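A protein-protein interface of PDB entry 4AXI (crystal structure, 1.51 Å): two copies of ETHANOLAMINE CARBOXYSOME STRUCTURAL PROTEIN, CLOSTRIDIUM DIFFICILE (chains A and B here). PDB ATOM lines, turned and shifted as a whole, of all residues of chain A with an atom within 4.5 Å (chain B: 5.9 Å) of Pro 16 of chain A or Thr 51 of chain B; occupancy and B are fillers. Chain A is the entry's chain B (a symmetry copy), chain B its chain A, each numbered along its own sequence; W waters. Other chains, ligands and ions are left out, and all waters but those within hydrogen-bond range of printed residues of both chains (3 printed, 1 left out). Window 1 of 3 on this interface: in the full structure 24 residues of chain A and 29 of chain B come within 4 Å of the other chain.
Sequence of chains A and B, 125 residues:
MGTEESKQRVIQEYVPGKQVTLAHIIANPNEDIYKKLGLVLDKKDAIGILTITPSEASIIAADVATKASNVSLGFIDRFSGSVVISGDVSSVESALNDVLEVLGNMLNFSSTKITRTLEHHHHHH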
ATOM      1  N   VAL A  15       0.407 -28.417 -24.501  1.00  0.00           N
ATOM      2  CA  VAL A  15      -0.557 -28.399 -23.402  1.00  0.00           C
ATOM      3  C   VAL A  15      -1.649 -27.439 -23.856  1.00  0.00           C
ATOM      4  O   VAL A  15      -1.409 -26.539 -24.653  1.00  0.00           O
ATOM      5  CB  VAL A  15       0.084 -27.924 -22.070  1.00  0.00           C
ATOM      6  CG1 VAL A  15       1.256 -28.777 -21.659  1.00  0.00           C
ATOM      7  CG2 VAL A  15       0.536 -26.463 -22.177  1.00  0.00           C
ATOM      8  N   PRO A  16      -2.867 -27.624 -23.346  1.00  0.00           N
ATOM      9  CA  PRO A  16      -3.894 -26.665 -23.726  1.00  0.00           C
ATOM     10  C   PRO A  16      -3.664 -25.298 -23.053  1.00  0.00           C
ATOM     11  O   PRO A  16      -3.261 -25.225 -21.898  1.00  0.00           O
ATOM     12  CB  PRO A  16      -5.182 -27.346 -23.222  1.00  0.00           C
ATOM     13  CG  PRO A  16      -4.740 -28.212 -22.094  1.00  0.00           C
ATOM     14  CD  PRO A  16      -3.380 -28.706 -22.480  1.00  0.00           C
ATOM     15  N   GLY A  17      -3.945 -24.224 -23.801  1.00  0.00           N
ATOM     16  CA  GLY A  17      -4.071 -22.890 -23.255  1.00  0.00           C
ATOM     17  C   GLY A  17      -5.374 -22.722 -22.487  1.00  0.00           C
ATOM     18  O   GLY A  17      -6.194 -23.645 -22.387  1.00  0.00           O
ATOM     19  N   LYS A  18      -5.497 -21.550 -21.896  1.00  0.00           N
ATOM     20  CA  LYS A  18      -6.677 -21.145 -21.143  1.00  0.00           C
ATOM     21  C   LYS A  18      -7.194 -19.889 -21.828  1.00  0.00           C
ATOM     22  O   LYS A  18      -6.626 -18.777 -21.681  1.00  0.00           O
ATOM     23  CB  LYS A  18      -6.260 -20.908 -19.670  1.00  0.00           C
ATOM     24  CG  LYS A  18      -5.780 -22.144 -19.014  1.00  0.00           C
ATOM     25  CD  LYS A  18      -5.376 -21.881 -17.579  1.00  0.00           C
ATOM     26  CE  LYS A  18      -3.966 -21.313 -17.487  1.00  0.00           C
ATOM     27  NZ  LYS A  18      -2.752 -22.258 -17.826  1.00  0.00           N
ATOM     28  N   THR A  53     -10.992 -23.172 -24.363  1.00  0.00           N
ATOM     29  CA  THR A  53      -9.872 -24.086 -24.165  1.00  0.00           C
ATOM     30  C   THR A  53      -9.406 -23.840 -22.744  1.00  0.00           C
ATOM     31  O   THR A  53      -9.345 -22.713 -22.338  1.00  0.00           O
ATOM     32  CB  THR A  53      -8.710 -23.716 -25.114  1.00  0.00           C
ATOM     33  OG1 THR A  53      -9.207 -23.608 -26.473  1.00  0.00           O
ATOM     34  CG2 THR A  53      -7.627 -24.743 -25.009  1.00  0.00           C
ATOM     35  N   PRO A  54      -9.130 -24.870 -21.949  1.00  0.00           N
ATOM     36  CA  PRO A  54      -9.249 -26.290 -22.330  1.00  0.00           C
ATOM     37  C   PRO A  54     -10.709 -26.715 -22.428  1.00  0.00           C
ATOM     38  O   PRO A  54     -11.621 -26.082 -21.844  1.00  0.00           O
ATOM     39  CB  PRO A  54      -8.587 -27.014 -21.153  1.00  0.00           C
ATOM     40  CG  PRO A  54      -8.874 -26.082 -19.979  1.00  0.00           C
ATOM     41  CD  PRO A  54      -8.655 -24.691 -20.564  1.00  0.00           C
ATOM     42  N   GLU A  56     -12.528 -28.970 -21.180  1.00  0.00           N
ATOM     43  CA  GLU A  56     -13.283 -29.287 -19.966  1.00  0.00           C
ATOM     44  C   GLU A  56     -13.928 -28.052 -19.341  1.00  0.00           C
ATOM     45  O   GLU A  56     -14.915 -28.163 -18.599  1.00  0.00           O
ATOM     46  CB  GLU A  56     -12.377 -29.941 -18.918  1.00  0.00           C
ATOM     47  CG  GLU A  56     -11.778 -31.274 -19.249  1.00  0.00           C
ATOM     48  CD  GLU A  56     -10.591 -31.279 -20.216  1.00  0.00           C
ATOM     49  OE1 GLU A  56     -10.038 -30.184 -20.545  1.00  0.00           O
ATOM     50  OE2 GLU A  56     -10.138 -32.411 -20.586  1.00  0.00           O
ATOM     51  N   GLN B  19       1.221 -31.520 -17.557  1.00  0.00           N
ATOM     52  CA  GLN B  19       0.520 -30.358 -16.981  1.00  0.00           C
ATOM     53  C   GLN B  19      -0.880 -30.719 -16.493  1.00  0.00           C
ATOM     54  O   GLN B  19      -1.630 -31.410 -17.203  1.00  0.00           O
ATOM     55  CB  GLN B  19       0.402 -29.283 -18.042  1.00  0.00           C
ATOM     56  CG  GLN B  19      -0.234 -27.971 -17.489  1.00  0.00           C
ATOM     57  CD  GLN B  19      -0.003 -26.808 -18.391  1.00  0.00           C
ATOM     58  OE1 GLN B  19       1.141 -26.360 -18.532  1.00  0.00           O
ATOM     59  NE2 GLN B  19      -1.075 -26.285 -19.006  1.00  0.00           N
ATOM     60  N   VAL B  20      -1.254 -30.224 -15.308  1.00  0.00           N
ATOM     61  CA  VAL B  20      -2.657 -30.166 -14.891  1.00  0.00           C
ATOM     62  C   VAL B  20      -3.105 -28.711 -15.119  1.00  0.00           C
ATOM     63  O   VAL B  20      -2.563 -27.779 -14.493  1.00  0.00           O
ATOM     64  CB  VAL B  20      -2.832 -30.551 -13.419  1.00  0.00           C
ATOM     65  CG1 VAL B  20      -4.317 -30.518 -13.057  1.00  0.00           C
ATOM     66  CG2 VAL B  20      -2.143 -31.879 -13.106  1.00  0.00           C
ATOM     67  N   THR B  21      -3.946 -28.487 -16.137  1.00  0.00           N
ATOM     68  CA  THR B  21      -4.312 -27.145 -16.531  1.00  0.00           C
ATOM     69  C   THR B  21      -5.447 -26.592 -15.715  1.00  0.00           C
ATOM     70  O   THR B  21      -5.558 -25.378 -15.560  1.00  0.00           O
ATOM     71  CB  THR B  21      -4.678 -27.134 -18.029  1.00  0.00           C
ATOM     72  OG1 THR B  21      -3.572 -27.598 -18.794  1.00  0.00           O
ATOM     73  CG2 THR B  21      -5.071 -25.795 -18.534  1.00  0.00           C
ATOM     74  N   LEU B  22      -6.279 -27.483 -15.195  1.00  0.00           N
ATOM     75  CA  LEU B  22      -7.493 -27.099 -14.485  1.00  0.00           C
ATOM     76  C   LEU B  22      -7.788 -28.098 -13.406  1.00  0.00           C
ATOM     77  O   LEU B  22      -7.699 -29.292 -13.612  1.00  0.00           O
ATOM     78  CB  LEU B  22      -8.651 -27.081 -15.495  1.00  0.00           C
ATOM     79  CG  LEU B  22     -10.042 -26.646 -15.087  1.00  0.00           C
ATOM     80  CD1 LEU B  22     -10.094 -25.155 -14.828  1.00  0.00           C
ATOM     81  CD2 LEU B  22     -11.053 -26.970 -16.221  1.00  0.00           C
ATOM     82  N   ALA B  23      -8.212 -27.573 -12.241  1.00  0.00           N
ATOM     83  CA  ALA B  23      -8.626 -28.388 -11.107  1.00  0.00           C
ATOM     84  C   ALA B  23      -9.709 -27.561 -10.426  1.00  0.00           C
ATOM     85  O   ALA B  23      -9.427 -26.739  -9.563  1.00  0.00           O
ATOM     86  CB  ALA B  23      -7.449 -28.687 -10.170  1.00  0.00           C
ATOM     87  N   ILE B  49     -13.422 -31.068 -11.545  1.00  0.00           N
ATOM     88  CA  ILE B  49     -13.060 -31.209 -12.964  1.00  0.00           C
ATOM     89  C   ILE B  49     -11.579 -31.037 -13.151  1.00  0.00           C
ATOM     90  O   ILE B  49     -11.030 -30.019 -12.733  1.00  0.00           O
ATOM     91  CB  ILE B  49     -13.799 -30.126 -13.763  1.00  0.00           C
ATOM     92  CG1 ILE B  49     -15.303 -30.263 -13.527  1.00  0.00           C
ATOM     93  CG2 ILE B  49     -13.465 -30.178 -15.284  1.00  0.00           C
ATOM     94  CD1 ILE B  49     -16.018 -28.991 -13.853  1.00  0.00           C
ATOM     95  N   LEU B  50     -10.953 -31.997 -13.854  1.00  0.00           N
ATOM     96  CA  LEU B  50      -9.525 -32.015 -14.111  1.00  0.00           C
ATOM     97  C   LEU B  50      -9.228 -32.043 -15.609  1.00  0.00           C
ATOM     98  O   LEU B  50      -9.857 -32.804 -16.340  1.00  0.00           O
ATOM     99  CB  LEU B  50      -8.864 -33.234 -13.462  1.00  0.00           C
ATOM    100  CG  LEU B  50      -8.735 -33.100 -11.940  1.00  0.00           C
ATOM    101  CD1 LEU B  50      -8.604 -34.426 -11.316  1.00  0.00           C
ATOM    102  CD2 LEU B  50      -7.462 -32.324 -11.591  1.00  0.00           C
ATOM    103  N   THR B  51      -8.248 -31.239 -16.020  1.00  0.00           N
ATOM    104  CA  THR B  51      -7.665 -31.243 -17.368  1.00  0.00           C
ATOM    105  C   THR B  51      -6.235 -31.691 -17.188  1.00  0.00           C
ATOM    106  O   THR B  51      -5.493 -31.029 -16.458  1.00  0.00           O
ATOM    107  CB  THR B  51      -7.665 -29.835 -17.959  1.00  0.00           C
ATOM    108  OG1 THR B  51      -8.999 -29.392 -18.116  1.00  0.00           O
ATOM    109  CG2 THR B  51      -6.981 -29.788 -19.317  1.00  0.00           C
ATOM    110  N   ILE B  52      -5.841 -32.780 -17.844  1.00  0.00           N
ATOM    111  CA  ILE B  52      -4.542 -33.382 -17.624  1.00  0.00           C
ATOM    112  C   ILE B  52      -3.889 -33.734 -18.942  1.00  0.00           C
ATOM    113  O   ILE B  52      -4.525 -34.323 -19.841  1.00  0.00           O
ATOM    114  CB  ILE B  52      -4.699 -34.693 -16.777  1.00  0.00           C
ATOM    115  CG1 ILE B  52      -5.298 -34.348 -15.383  1.00  0.00           C
ATOM    116  CG2 ILE B  52      -3.349 -35.382 -16.596  1.00  0.00           C
ATOM    117  CD1 ILE B  52      -5.877 -35.519 -14.743  1.00  0.00           C
ATOM    118  N   THR B  53      -2.591 -33.457 -19.061  1.00  0.00           N
ATOM    119  CA  THR B  53      -1.764 -33.861 -20.202  1.00  0.00           C
ATOM    120  C   THR B  53      -0.476 -34.465 -19.576  1.00  0.00           C
ATOM    121  O   THR B  53       0.033 -33.923 -18.634  1.00  0.00           O
ATOM    122  CB  THR B  53      -1.363 -32.645 -21.044  1.00  0.00           C
ATOM    123  OG1 THR B  53      -2.533 -31.856 -21.403  1.00  0.00           O
ATOM    124  CG2 THR B  53      -0.614 -33.089 -22.294  1.00  0.00           C
ATOM    125  N   GLY B  81      -7.860 -36.970 -21.486  1.00  0.00           N
ATOM    126  CA  GLY B  81      -7.243 -36.632 -20.201  1.00  0.00           C
ATOM    127  C   GLY B  81      -8.178 -36.206 -19.092  1.00  0.00           C
ATOM    128  O   GLY B  81      -7.784 -36.030 -17.930  1.00  0.00           O
ATOM    129  N   SER B  82      -9.431 -36.063 -19.430  1.00  0.00           N
ATOM    130  CA  SER B  82     -10.381 -35.471 -18.501  1.00  0.00           C
ATOM    131  C   SER B  82     -10.736 -36.423 -17.373  1.00  0.00           C
ATOM    132  O   SER B  82     -10.919 -37.620 -17.570  1.00  0.00           O
ATOM    133  CB  SER B  82     -11.688 -35.137 -19.221  1.00  0.00           C
ATOM    134  OG  SER B  82     -11.476 -34.489 -20.470  1.00  0.00           O
ATOM    135  N   VAL B  83     -10.936 -35.847 -16.194  1.00  0.00           N
ATOM    136  CA  VAL B  83     -11.448 -36.599 -15.065  1.00  0.00           C
ATOM    137  C   VAL B  83     -12.464 -35.708 -14.352  1.00  0.00           C
ATOM    138  O   VAL B  83     -12.202 -34.538 -14.077  1.00  0.00           O
ATOM    139  CB  VAL B  83     -10.335 -37.040 -14.068  1.00  0.00           C
ATOM    140  CG1 VAL B  83     -10.940 -37.732 -12.845  1.00  0.00           C
ATOM    141  CG2 VAL B  83      -9.287 -37.913 -14.709  1.00  0.00           C
HETATM  142  O   HOH W   1      -7.512 -33.159 -20.159  1.00  0.00           O
HETATM  143  O   HOH W   2      -1.907 -23.679 -20.192  1.00  0.00           O
HETATM  144  O   HOH W   3      -3.405 -23.385 -15.301  1.00  0.00           O
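Among the printed residues, pairs that only touch across the chains: Pro 16 of chain A with Thr 53 of chain B, Pro 16 of chain A with Thr 21 of chain B, Val 15 of chain A with Gln 19 of chain B, Pro 54 of chain A with Thr 51 of chain B, Lys 18 of chain A with Thr 21 of chain B, Pro 16 of chain A with Gln 19 of chain B, Glu 56 of chain A with Ile 49 of chain B, Glu 56 of chain A with Leu 50 of chain B and Pro 16 of chain A with Thr 51 of chain B.
Water W2 lies within hydrogen-bond range of the backbone carbonyl oxygen of Pro 16 of chain A (2.7 Å), the side-chain amino group of Lys 18 of chain A (2.9 Å) and the side-chain amide nitrogen of Gln 19 of chain B (3.0 Å). Water W1 bridges the side-chain carboxylate (OE2) of Glu 56 of chain A and the backbone NH (N) of Ile 52 of chain B. Water W3 lies within hydrogen-bond range of NZ of Lys 18 of chain A and O of Thr 21 of chain B.
Of chain B, only Gln 19, Thr 21, Thr 51 and Thr 53 come within 4 Å of Pro 16 of chain A. Of the printed residues of chain B, Pro 54 of chain A touches Thr 51 (3.7 Å). Ala 23 of chain B touches none of the printed residues of chain A. Printed residues of chain A within 4 Å of Ile 49 of chain B: Glu 56. Thr 51 of chain B touches just these residues of chain A: Pro 16, Pro 54 and Glu 56. Of the printed residues of chain A, Thr 53 of chain B touches Pro 16. The nearest printed residue of chain A that does not touch Thr 51 of chain B is Gly 17 of chain A (6.9 Å). The nearest printed residue of chain B that does not touch Val 15 of chain A is Thr 53 of chain B (4.5 Å).
N of Thr 21 of chain B is in hydrogen-bond range of O of Thr 51 of chain B, at 3.0 Å. The side-chain hydroxyl of Thr 21 of chain B is in hydrogen-bond range of the side-chain amide nitrogen of Gln 19 of chain B (2.8 Å). O of Leu 22 of chain B is in hydrogen-bond range of N of Thr 51 of chain B. The backbone carbonyl oxygen (O) of Thr 53 of chain B sits at hydrogen-bond distance from the backbone NH (N) of Gln 19 of chain B, 2.9 Å away. O of Val 83 of chain B sits at hydrogen-bond distance from N of Leu 50 of chain B (2.8 Å).
1 position is printed for both chains. Of the 11 pairs that touch across the chains among the printed residues, none has its exchanged pair printed and touching as well.
The side-chain hydroxyl (OG) of Ser 82 of chain B sits at hydrogen-bond distance from the side-chain carboxylate (OE2) of Glu 56 of chain A, 2.5 Å away. The side-chain hydroxyl of Thr 51 of chain B lies within hydrogen-bond range of the side-chain carboxylate of Glu 56 of chain A, at 2.8 Å.
Hydrophobic or aromatic side chains of chain A within 4 Å of the printed part of chain B: Val 15, Pro 16 and Pro 54. Among the printed residues, 11 pairs touch across the chains.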
